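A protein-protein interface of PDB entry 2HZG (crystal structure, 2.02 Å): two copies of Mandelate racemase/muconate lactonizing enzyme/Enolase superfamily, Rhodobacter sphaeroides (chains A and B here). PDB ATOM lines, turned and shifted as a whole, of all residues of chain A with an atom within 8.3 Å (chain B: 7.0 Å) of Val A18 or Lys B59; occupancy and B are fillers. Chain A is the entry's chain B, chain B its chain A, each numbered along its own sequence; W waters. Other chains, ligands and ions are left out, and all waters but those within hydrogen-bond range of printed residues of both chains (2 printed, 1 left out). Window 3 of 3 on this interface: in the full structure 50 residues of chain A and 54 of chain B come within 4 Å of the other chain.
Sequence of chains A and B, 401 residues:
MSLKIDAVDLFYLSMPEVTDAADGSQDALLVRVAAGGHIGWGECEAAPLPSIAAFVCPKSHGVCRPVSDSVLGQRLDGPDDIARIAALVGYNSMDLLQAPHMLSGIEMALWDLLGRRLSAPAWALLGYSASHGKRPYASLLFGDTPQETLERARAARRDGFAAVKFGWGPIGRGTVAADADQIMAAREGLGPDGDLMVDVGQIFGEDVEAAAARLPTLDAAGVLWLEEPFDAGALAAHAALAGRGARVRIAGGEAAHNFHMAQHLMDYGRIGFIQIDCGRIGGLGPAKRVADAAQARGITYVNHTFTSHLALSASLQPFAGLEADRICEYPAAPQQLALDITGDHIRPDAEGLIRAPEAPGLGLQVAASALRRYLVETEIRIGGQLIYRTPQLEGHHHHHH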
ATOM      1  N   TYR A  12      -3.451  -9.519 -35.567  1.00  0.00           N
ATOM      2  CA  TYR A  12      -3.633 -10.208 -34.295  1.00  0.00           C
ATOM      3  C   TYR A  12      -4.464  -9.280 -33.416  1.00  0.00           C
ATOM      4  O   TYR A  12      -4.002  -8.215 -33.039  1.00  0.00           O
ATOM      5  CB  TYR A  12      -2.262 -10.483 -33.649  1.00  0.00           C
ATOM      6  CG  TYR A  12      -2.222 -11.373 -32.416  1.00  0.00           C
ATOM      7  CD1 TYR A  12      -0.995 -11.893 -31.978  1.00  0.00           C
ATOM      8  CD2 TYR A  12      -3.377 -11.707 -31.695  1.00  0.00           C
ATOM      9  CE1 TYR A  12      -0.905 -12.708 -30.854  1.00  0.00           C
ATOM     10  CE2 TYR A  12      -3.305 -12.526 -30.547  1.00  0.00           C
ATOM     11  CZ  TYR A  12      -2.053 -13.023 -30.139  1.00  0.00           C
ATOM     12  OH  TYR A  12      -1.933 -13.864 -29.057  1.00  0.00           O
ATOM     13  N   LEU A  13      -5.687  -9.689 -33.098  1.00  0.00           N
ATOM     14  CA  LEU A  13      -6.586  -8.880 -32.270  1.00  0.00           C
ATOM     15  C   LEU A  13      -6.826  -9.598 -30.962  1.00  0.00           C
ATOM     16  O   LEU A  13      -6.944 -10.806 -30.953  1.00  0.00           O
ATOM     17  CB  LEU A  13      -7.923  -8.678 -32.978  1.00  0.00           C
ATOM     18  CG  LEU A  13      -7.891  -8.018 -34.360  1.00  0.00           C
ATOM     19  CD1 LEU A  13      -9.321  -7.723 -34.786  1.00  0.00           C
ATOM     20  CD2 LEU A  13      -7.075  -6.732 -34.338  1.00  0.00           C
ATOM     21  N   SER A  14      -6.896  -8.855 -29.862  1.00  0.00           N
ATOM     22  CA  SER A  14      -7.169  -9.451 -28.556  1.00  0.00           C
ATOM     23  C   SER A  14      -7.939  -8.485 -27.667  1.00  0.00           C
ATOM     24  O   SER A  14      -7.746  -7.275 -27.756  1.00  0.00           O
ATOM     25  CB  SER A  14      -5.854  -9.874 -27.868  1.00  0.00           C
ATOM     26  OG  SER A  14      -6.105 -10.608 -26.663  1.00  0.00           O
ATOM     27  N   MET A  15      -8.831  -9.034 -26.840  1.00  0.00           N
ATOM     28  CA  MET A  15      -9.351  -8.351 -25.662  1.00  0.00           C
ATOM     29  C   MET A  15      -8.158  -8.036 -24.752  1.00  0.00           C
ATOM     30  O   MET A  15      -7.181  -8.791 -24.764  1.00  0.00           O
ATOM     31  CB  MET A  15     -10.325  -9.264 -24.915  1.00  0.00           C
ATOM     32  CG  MET A  15     -11.635  -9.551 -25.657  1.00  0.00           C
ATOM     33  SD  MET A  15     -12.612  -8.062 -25.867  1.00  0.00           S
ATOM     34  CE  MET A  15     -13.138  -7.768 -24.170  1.00  0.00           C
ATOM     35  N   PRO A  16      -8.231  -6.933 -23.964  1.00  0.00           N
ATOM     36  CA  PRO A  16      -7.099  -6.478 -23.125  1.00  0.00           C
ATOM     37  C   PRO A  16      -6.652  -7.512 -22.095  1.00  0.00           C
ATOM     38  O   PRO A  16      -5.453  -7.598 -21.785  1.00  0.00           O
ATOM     39  CB  PRO A  16      -7.646  -5.232 -22.403  1.00  0.00           C
ATOM     40  CG  PRO A  16      -8.889  -4.866 -23.090  1.00  0.00           C
ATOM     41  CD  PRO A  16      -9.413  -6.059 -23.817  1.00  0.00           C
ATOM     42  N   GLU A  17      -7.609  -8.273 -21.569  1.00  0.00           N
ATOM     43  CA  GLU A  17      -7.320  -9.381 -20.663  1.00  0.00           C
ATOM     44  C   GLU A  17      -7.905 -10.651 -21.264  1.00  0.00           C
ATOM     45  O   GLU A  17      -9.077 -10.671 -21.687  1.00  0.00           O
ATOM     46  CB  GLU A  17      -7.941  -9.138 -19.277  1.00  0.00           C
ATOM     47  CG  GLU A  17      -7.346  -7.965 -18.519  1.00  0.00           C
ATOM     48  CD  GLU A  17      -7.736  -7.943 -17.038  1.00  0.00           C
ATOM     49  OE1 GLU A  17      -7.802  -9.030 -16.397  1.00  0.00           O
ATOM     50  OE2 GLU A  17      -7.972  -6.827 -16.506  1.00  0.00           O
ATOM     51  N   VAL A  18      -7.085 -11.691 -21.350  1.00  0.00           N
ATOM     52  CA  VAL A  18      -7.533 -12.980 -21.853  1.00  0.00           C
ATOM     53  C   VAL A  18      -7.522 -13.917 -20.661  1.00  0.00           C
ATOM     54  O   VAL A  18      -6.540 -13.970 -19.937  1.00  0.00           O
ATOM     55  CB  VAL A  18      -6.634 -13.491 -23.016  1.00  0.00           C
ATOM     56  CG1 VAL A  18      -6.967 -14.930 -23.392  1.00  0.00           C
ATOM     57  CG2 VAL A  18      -6.779 -12.570 -24.230  1.00  0.00           C
ATOM     58  N   THR A  19      -8.625 -14.629 -20.450  1.00  0.00           N
ATOM     59  CA  THR A  19      -8.758 -15.532 -19.314  1.00  0.00           C
ATOM     60  C   THR A  19      -8.756 -16.997 -19.743  1.00  0.00           C
ATOM     61  O   THR A  19      -8.801 -17.312 -20.941  1.00  0.00           O
ATOM     62  CB  THR A  19     -10.076 -15.284 -18.537  1.00  0.00           C
ATOM     63  OG1 THR A  19     -11.149 -15.928 -19.224  1.00  0.00           O
ATOM     64  CG2 THR A  19     -10.391 -13.779 -18.395  1.00  0.00           C
ATOM     65  N   ASP A  20      -8.728 -17.885 -18.746  1.00  0.00           N
ATOM     66  CA  ASP A  20      -8.767 -19.324 -18.962  1.00  0.00           C
ATOM     67  C   ASP A  20     -10.138 -19.869 -19.300  1.00  0.00           C
ATOM     68  O   ASP A  20     -10.266 -21.066 -19.512  1.00  0.00           O
ATOM     69  CB  ASP A  20      -8.223 -20.077 -17.748  1.00  0.00           C
ATOM     70  CG  ASP A  20      -6.712 -20.061 -17.695  1.00  0.00           C
ATOM     71  OD1 ASP A  20      -6.075 -20.037 -18.768  1.00  0.00           O
ATOM     72  OD2 ASP A  20      -6.167 -20.047 -16.575  1.00  0.00           O
ATOM     73  N   ALA A  21     -11.161 -19.012 -19.330  1.00  0.00           N
ATOM     74  CA  ALA A  21     -12.474 -19.408 -19.852  1.00  0.00           C
ATOM     75  C   ALA A  21     -12.348 -20.135 -21.197  1.00  0.00           C
ATOM     76  O   ALA A  21     -11.469 -19.835 -22.006  1.00  0.00           O
ATOM     77  CB  ALA A  21     -13.379 -18.192 -20.013  1.00  0.00           C
ATOM     78  N   ASP A  23     -13.478 -19.776 -23.969  1.00  0.00           N
ATOM     79  CA  ASP A  23     -14.118 -18.778 -24.820  1.00  0.00           C
ATOM     80  C   ASP A  23     -13.142 -18.338 -25.923  1.00  0.00           C
ATOM     81  O   ASP A  23     -12.207 -17.569 -25.687  1.00  0.00           O
ATOM     82  CB  ASP A  23     -14.558 -17.592 -23.953  1.00  0.00           C
ATOM     83  CG  ASP A  23     -15.330 -16.519 -24.723  1.00  0.00           C
ATOM     84  OD1 ASP A  23     -15.393 -16.561 -25.976  1.00  0.00           O
ATOM     85  OD2 ASP A  23     -15.882 -15.617 -24.040  1.00  0.00           O
ATOM     86  N   GLY A  24     -13.389 -18.840 -27.131  1.00  0.00           N
ATOM     87  CA  GLY A  24     -12.560 -18.541 -28.279  1.00  0.00           C
ATOM     88  C   GLY A  24     -12.811 -17.192 -28.925  1.00  0.00           C
ATOM     89  O   GLY A  24     -12.166 -16.860 -29.914  1.00  0.00           O
ATOM     90  N   SER A  25     -13.712 -16.384 -28.369  1.00  0.00           N
ATOM     91  CA  SER A  25     -13.922 -15.034 -28.922  1.00  0.00           C
ATOM     92  C   SER A  25     -13.061 -13.952 -28.251  1.00  0.00           C
ATOM     93  O   SER A  25     -13.165 -12.763 -28.588  1.00  0.00           O
ATOM     94  CB  SER A  25     -15.406 -14.646 -28.902  1.00  0.00           C
ATOM     95  OG  SER A  25     -15.884 -14.467 -27.573  1.00  0.00           O
ATOM     96  N   GLN A  26     -12.185 -14.363 -27.341  1.00  0.00           N
ATOM     97  CA  GLN A  26     -11.303 -13.424 -26.656  1.00  0.00           C
ATOM     98  C   GLN A  26     -10.181 -12.876 -27.525  1.00  0.00           C
ATOM     99  O   GLN A  26      -9.583 -11.857 -27.187  1.00  0.00           O
ATOM    100  CB  GLN A  26     -10.699 -14.068 -25.414  1.00  0.00           C
ATOM    101  CG  GLN A  26     -11.708 -14.668 -24.472  1.00  0.00           C
ATOM    102  CD  GLN A  26     -11.045 -15.144 -23.201  1.00  0.00           C
ATOM    103  OE1 GLN A  26     -10.670 -14.336 -22.359  1.00  0.00           O
ATOM    104  NE2 GLN A  26     -10.891 -16.458 -23.060  1.00  0.00           N
ATOM    105  N   ASP A  27      -9.855 -13.577 -28.611  1.00  0.00           N
ATOM    106  CA  ASP A  27      -8.881 -13.051 -29.581  1.00  0.00           C
ATOM    107  C   ASP A  27      -9.234 -13.531 -30.986  1.00  0.00           C
ATOM    108  O   ASP A  27     -10.183 -14.283 -31.150  1.00  0.00           O
ATOM    109  CB  ASP A  27      -7.424 -13.362 -29.173  1.00  0.00           C
ATOM    110  CG  ASP A  27      -7.029 -14.842 -29.388  1.00  0.00           C
ATOM    111  OD1 ASP A  27      -7.888 -15.677 -29.729  1.00  0.00           O
ATOM    112  OD2 ASP A  27      -5.838 -15.165 -29.200  1.00  0.00           O
ATOM    113  N   ALA A  28      -8.501 -13.072 -32.000  1.00  0.00           N
ATOM    114  CA  ALA A  28      -8.807 -13.419 -33.383  1.00  0.00           C
ATOM    115  C   ALA A  28      -7.602 -13.099 -34.238  1.00  0.00           C
ATOM    116  O   ALA A  28      -6.798 -12.211 -33.911  1.00  0.00           O
ATOM    117  CB  ALA A  28     -10.013 -12.614 -33.881  1.00  0.00           C
ATOM    118  N   ALA A  47      -4.951 -20.196 -32.903  1.00  0.00           N
ATOM    119  CA  ALA A  47      -3.903 -19.454 -32.178  1.00  0.00           C
ATOM    120  C   ALA A  47      -3.255 -18.432 -33.139  1.00  0.00           C
ATOM    121  O   ALA A  47      -2.616 -18.827 -34.116  1.00  0.00           O
ATOM    122  CB  ALA A  47      -2.886 -20.450 -31.699  1.00  0.00           C
ATOM    123  N   PRO A  48      -3.474 -17.119 -32.917  1.00  0.00           N
ATOM    124  CA  PRO A  48      -3.012 -16.117 -33.875  1.00  0.00           C
ATOM    125  C   PRO A  48      -1.501 -16.072 -34.151  1.00  0.00           C
ATOM    126  O   PRO A  48      -1.124 -16.015 -35.316  1.00  0.00           O
ATOM    127  CB  PRO A  48      -3.522 -14.795 -33.264  1.00  0.00           C
ATOM    128  CG  PRO A  48      -4.714 -15.213 -32.498  1.00  0.00           C
ATOM    129  CD  PRO A  48      -4.272 -16.492 -31.852  1.00  0.00           C
ATOM    130  N   LEU A  49      -0.655 -16.131 -33.119  1.00  0.00           N
ATOM    131  CA  LEU A  49       0.793 -16.087 -33.346  1.00  0.00           C
ATOM    132  C   LEU A  49       1.376 -17.317 -34.075  1.00  0.00           C
ATOM    133  O   LEU A  49       2.123 -17.155 -35.040  1.00  0.00           O
ATOM    134  CB  LEU A  49       1.581 -15.787 -32.061  1.00  0.00           C
ATOM    135  CG  LEU A  49       3.105 -15.667 -32.239  1.00  0.00           C
ATOM    136  CD1 LEU A  49       3.459 -14.439 -33.113  1.00  0.00           C
ATOM    137  CD2 LEU A  49       3.778 -15.587 -30.863  1.00  0.00           C
ATOM    138  N   GLN A 335     -17.327 -12.139 -26.773  1.00  0.00           N
ATOM    139  CA  GLN A 335     -16.618 -10.974 -26.278  1.00  0.00           C
ATOM    140  C   GLN A 335     -16.844  -9.770 -27.188  1.00  0.00           C
ATOM    141  O   GLN A 335     -17.138  -9.921 -28.381  1.00  0.00           O
ATOM    142  CB  GLN A 335     -15.117 -11.269 -26.142  1.00  0.00           C
ATOM    143  CG  GLN A 335     -14.819 -12.414 -25.194  1.00  0.00           C
ATOM    144  CD  GLN A 335     -15.048 -12.027 -23.744  1.00  0.00           C
ATOM    145  OE1 GLN A 335     -14.902 -10.866 -23.373  1.00  0.00           O
ATOM    146  NE2 GLN A 335     -15.410 -12.994 -22.924  1.00  0.00           N
ATOM    147  N   LEU A 337     -14.817  -7.857 -28.567  1.00  0.00           N
ATOM    148  CA  LEU A 337     -13.975  -7.934 -29.759  1.00  0.00           C
ATOM    149  C   LEU A 337     -14.765  -8.518 -30.951  1.00  0.00           C
ATOM    150  O   LEU A 337     -14.750  -7.959 -32.056  1.00  0.00           O
ATOM    151  CB  LEU A 337     -12.727  -8.783 -29.480  1.00  0.00           C
ATOM    152  CG  LEU A 337     -11.887  -9.221 -30.692  1.00  0.00           C
ATOM    153  CD1 LEU A 337     -11.368  -8.031 -31.544  1.00  0.00           C
ATOM    154  CD2 LEU A 337     -10.751 -10.154 -30.249  1.00  0.00           C
ATOM    155  N   VAL A 376      -2.824  -6.284 -31.506  1.00  0.00           N
ATOM    156  CA  VAL A 376      -1.687  -6.745 -30.711  1.00  0.00           C
ATOM    157  C   VAL A 376      -0.420  -6.411 -31.485  1.00  0.00           C
ATOM    158  O   VAL A 376      -0.256  -6.870 -32.616  1.00  0.00           O
ATOM    159  CB  VAL A 376      -1.756  -8.266 -30.413  1.00  0.00           C
ATOM    160  CG1 VAL A 376      -0.491  -8.738 -29.690  1.00  0.00           C
ATOM    161  CG2 VAL A 376      -3.003  -8.588 -29.607  1.00  0.00           C
ATOM    162  N   VAL B  56       5.548 -20.436 -26.963  1.00  0.00           N
ATOM    163  CA  VAL B  56       5.598 -19.170 -26.211  1.00  0.00           C
ATOM    164  C   VAL B  56       4.430 -18.204 -26.422  1.00  0.00           C
ATOM    165  O   VAL B  56       4.409 -17.153 -25.806  1.00  0.00           O
ATOM    166  CB  VAL B  56       6.910 -18.365 -26.521  1.00  0.00           C
ATOM    167  CG1 VAL B  56       8.165 -19.225 -26.174  1.00  0.00           C
ATOM    168  CG2 VAL B  56       6.946 -17.894 -28.008  1.00  0.00           C
ATOM    169  N   CYS B  57       3.494 -18.527 -27.317  1.00  0.00           N
ATOM    170  CA  CYS B  57       2.472 -17.553 -27.701  1.00  0.00           C
ATOM    171  C   CYS B  57       1.615 -17.082 -26.518  1.00  0.00           C
ATOM    172  O   CYS B  57       1.413 -17.825 -25.569  1.00  0.00           O
ATOM    173  CB  CYS B  57       1.556 -18.110 -28.809  1.00  0.00           C
ATOM    174  SG  CYS B  57       0.754 -19.652 -28.400  1.00  0.00           S
ATOM    175  N   PRO B  58       1.087 -15.850 -26.593  1.00  0.00           N
ATOM    176  CA  PRO B  58       0.055 -15.475 -25.619  1.00  0.00           C
ATOM    177  C   PRO B  58      -1.100 -16.473 -25.707  1.00  0.00           C
ATOM    178  O   PRO B  58      -1.415 -16.972 -26.798  1.00  0.00           O
ATOM    179  CB  PRO B  58      -0.401 -14.092 -26.112  1.00  0.00           C
ATOM    180  CG  PRO B  58       0.769 -13.540 -26.853  1.00  0.00           C
ATOM    181  CD  PRO B  58       1.368 -14.758 -27.544  1.00  0.00           C
ATOM    182  N   LYS B  59      -1.716 -16.823 -24.588  1.00  0.00           N
ATOM    183  CA  LYS B  59      -2.838 -17.753 -24.687  1.00  0.00           C
ATOM    184  C   LYS B  59      -4.019 -17.104 -25.426  1.00  0.00           C
ATOM    185  O   LYS B  59      -4.160 -15.867 -25.442  1.00  0.00           O
ATOM    186  CB  LYS B  59      -3.243 -18.290 -23.313  1.00  0.00           C
ATOM    187  CG  LYS B  59      -4.071 -17.328 -22.475  1.00  0.00           C
ATOM    188  CD  LYS B  59      -4.510 -17.965 -21.156  1.00  0.00           C
ATOM    189  CE  LYS B  59      -4.858 -16.846 -20.174  1.00  0.00           C
ATOM    190  NZ  LYS B  59      -4.582 -17.238 -18.759  1.00  0.00           N
ATOM    191  N   SER B  60      -4.847 -17.933 -26.051  1.00  0.00           N
ATOM    192  CA  SER B  60      -6.065 -17.457 -26.701  1.00  0.00           C
ATOM    193  C   SER B  60      -7.250 -17.623 -25.762  1.00  0.00           C
ATOM    194  O   SER B  60      -8.187 -16.827 -25.771  1.00  0.00           O
ATOM    195  CB  SER B  60      -6.313 -18.201 -28.024  1.00  0.00           C
ATOM    196  OG  SER B  60      -5.413 -17.716 -29.001  1.00  0.00           O
ATOM    197  N   HIS B  61      -7.176 -18.676 -24.963  1.00  0.00           N
ATOM    198  CA  HIS B  61      -8.188 -19.043 -23.978  1.00  0.00           C
ATOM    199  C   HIS B  61      -7.687 -20.306 -23.269  1.00  0.00           C
ATOM    200  O   HIS B  61      -6.542 -20.715 -23.493  1.00  0.00           O
ATOM    201  CB  HIS B  61      -9.572 -19.251 -24.629  1.00  0.00           C
ATOM    202  CG  HIS B  61      -9.599 -20.282 -25.712  1.00  0.00           C
ATOM    203  ND1 HIS B  61      -9.430 -19.967 -27.043  1.00  0.00           N
ATOM    204  CD2 HIS B  61      -9.799 -21.619 -25.664  1.00  0.00           C
ATOM    205  CE1 HIS B  61      -9.517 -21.071 -27.767  1.00  0.00           C
ATOM    206  NE2 HIS B  61      -9.751 -22.082 -26.955  1.00  0.00           N
ATOM    207  N   GLY B  62      -8.518 -20.891 -22.403  1.00  0.00           N
ATOM    208  CA  GLY B  62      -8.113 -21.999 -21.525  1.00  0.00           C
ATOM    209  C   GLY B  62      -7.638 -23.279 -22.185  1.00  0.00           C
ATOM    210  O   GLY B  62      -6.842 -24.022 -21.601  1.00  0.00           O
ATOM    211  N   CYS B  64      -6.384 -23.138 -25.404  1.00  0.00           N
ATOM    212  CA  CYS B  64      -5.423 -22.691 -26.402  1.00  0.00           C
ATOM    213  C   CYS B  64      -4.293 -21.890 -25.706  1.00  0.00           C
ATOM    214  O   CYS B  64      -4.098 -20.700 -25.944  1.00  0.00           O
ATOM    215  CB  CYS B  64      -6.127 -21.900 -27.508  1.00  0.00           C
ATOM    216  SG  CYS B  64      -5.143 -21.582 -28.969  1.00  0.00           S
ATOM    217  N   ARG B  65      -3.570 -22.570 -24.825  1.00  0.00           N
ATOM    218  CA  ARG B  65      -2.440 -21.973 -24.128  1.00  0.00           C
ATOM    219  C   ARG B  65      -1.149 -22.312 -24.847  1.00  0.00           C
ATOM    220  O   ARG B  65      -1.091 -23.317 -25.551  1.00  0.00           O
ATOM    221  CB  ARG B  65      -2.369 -22.531 -22.702  1.00  0.00           C
ATOM    222  CG  ARG B  65      -3.602 -22.236 -21.915  1.00  0.00           C
ATOM    223  CD  ARG B  65      -3.424 -22.555 -20.454  1.00  0.00           C
ATOM    224  NE  ARG B  65      -4.658 -23.134 -19.967  1.00  0.00           N
ATOM    225  CZ  ARG B  65      -4.969 -23.297 -18.682  1.00  0.00           C
ATOM    226  NH1 ARG B  65      -4.110 -22.911 -17.734  1.00  0.00           N
ATOM    227  NH2 ARG B  65      -6.141 -23.854 -18.352  1.00  0.00           N
ATOM    228  N   PRO B  66      -0.098 -21.502 -24.635  1.00  0.00           N
ATOM    229  CA  PRO B  66       1.223 -21.875 -25.152  1.00  0.00           C
ATOM    230  C   PRO B  66       1.651 -23.198 -24.532  1.00  0.00           C
ATOM    231  O   PRO B  66       1.327 -23.478 -23.370  1.00  0.00           O
ATOM    232  CB  PRO B  66       2.129 -20.744 -24.652  1.00  0.00           C
ATOM    233  CG  PRO B  66       1.388 -20.184 -23.404  1.00  0.00           C
ATOM    234  CD  PRO B  66      -0.055 -20.235 -23.874  1.00  0.00           C
ATOM    235  N   ASP B  69       3.148 -23.386 -20.841  1.00  0.00           N
ATOM    236  CA  ASP B  69       2.249 -23.369 -19.662  1.00  0.00           C
ATOM    237  C   ASP B  69       2.052 -24.740 -19.035  1.00  0.00           C
ATOM    238  O   ASP B  69       1.786 -24.847 -17.839  1.00  0.00           O
ATOM    239  CB  ASP B  69       0.862 -22.820 -20.042  1.00  0.00           C
ATOM    240  CG  ASP B  69       0.794 -21.298 -20.034  1.00  0.00           C
ATOM    241  OD1 ASP B  69       1.816 -20.624 -19.799  1.00  0.00           O
ATOM    242  OD2 ASP B  69      -0.313 -20.770 -20.286  1.00  0.00           O
ATOM    243  N   ASN B  92      -4.573 -28.395 -22.490  1.00  0.00           N
ATOM    244  CA  ASN B  92      -4.383 -26.933 -22.434  1.00  0.00           C
ATOM    245  C   ASN B  92      -4.078 -26.297 -23.792  1.00  0.00           C
ATOM    246  O   ASN B  92      -4.300 -25.099 -23.979  1.00  0.00           O
ATOM    247  CB  ASN B  92      -3.245 -26.553 -21.472  1.00  0.00           C
ATOM    248  CG  ASN B  92      -3.632 -26.686 -19.996  1.00  0.00           C
ATOM    249  OD1 ASN B  92      -4.808 -26.765 -19.658  1.00  0.00           O
ATOM    250  ND2 ASN B  92      -2.624 -26.679 -19.112  1.00  0.00           N
HETATM  251  O   HOH W   1      -5.835 -15.636 -17.105  1.00  0.00           O
HETATM  252  O   HOH W   2      -3.999 -14.177 -27.603  1.00  0.00           O
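The side-chain amino group of Lys B59 lies within salt-bridge range of the side-chain carboxylate of Asp A20. OD2 of Asp A27 is in hydrogen-bond range of OG of Ser B60, at 2.6 Å. The backbone NH (N) of Gly B62 lies close to the backbone carbonyl oxygen (O) of Asp A20, at 3.4 Å. The backbone NH (N) of Gly B62 is in hydrogen-bond range of the backbone carbonyl oxygen (O) of Ala A21. OD1 of Asp A20 lies within salt-bridge range of NE of Arg B65 (3.6 Å).
O of Gly B62 is in hydrogen-bond range of NE of Arg B65 (2.9 Å). The backbone NH of Arg B65 sits at hydrogen-bond distance from the backbone carbonyl oxygen of Asn B92 (2.8 Å). O of Tyr A12 is in hydrogen-bond range of N of Val A376, 2.7 Å away. N of Met A15 is in hydrogen-bond range of O of Gln A26 (2.9 Å). N of Ala A21 is in hydrogen-bond range of OG1 of Thr A19 (3.1 Å). OG of Ser A25 is in hydrogen-bond range of OD1 of Asp A23, 2.7 Å away.
Pro B58 touches Tyr A12 (CB to OH, 3.3 Å). Lys B59 touches Val A18. Thr A19 touches His B61. Thr A19 touches Gly B62. His B61 touches Ala A21. ND1 of His B61 touches CA of Gly A24, 3.7 Å away. CB of Gln A26 touches O of Ser B60, 3.7 Å away. His B61 touches Gln A26. Cys B64 touches Ala A47. Leu A49 touches Cys B57.
Val A18 touches two residues of chain B. Ser B60 touches just these residues of chain A: Val A18, Gln A26, Asp A27, Ala A47 and Pro A48. Of the printed residues of chain B, Asp A20 touches Lys B59 (3.2 Å), Gly B62 (3.1 Å) and Arg B65 (3.4 Å). Of the printed residues of chain A, Cys B57 touches Leu A49. The nearest printed residue of chain A that does not touch Cys B64 is Pro A48 (5.9 Å).
Printed residues of chain A that touch a printed residue of chain B: Tyr A12, Val A18, Thr A19, Asp A20, Ala A21, Asp A23, Gly A24, Gln A26, Asp A27, Ala A47, Pro A48 and Leu A49. Hydrophobic or aromatic side chains of chain A within 4 Å of the printed part of chain B: Tyr A12, Val A18, Ala A47, Pro A48 and Leu A49. Of the 12 printed residues of chain B, 8 touch a printed residue of chain A. Hydrophobic or aromatic side chains of chain B within 4 Å of the printed part of chain A: Pro B58 and His B61. Among the printed residues, 20 pairs touch across the chains. Among the printed residues, Asp or Glu carboxylates within 4 Å of a Lys or Arg side-chain nitrogen of the other chain: Asp A20 with Lys B59 and Asp A20 with Arg B65.
No position is printed for both chains. Of the 20 pairs that touch across the chains among the printed residues, none has its exchanged pair printed and touching as well.
Water W2 lies within hydrogen-bond range of the side-chain hydroxyl of Tyr A12 (2.5 Å), the side-chain carboxylate of Asp A27 (2.6 Å) and the backbone carbonyl oxygen of Lys B59 (2.7 Å). Water W1 lies within hydrogen-bond range of NZ of Lys B59 (2.6 Å) and O of Val A18 (3.4 Å).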
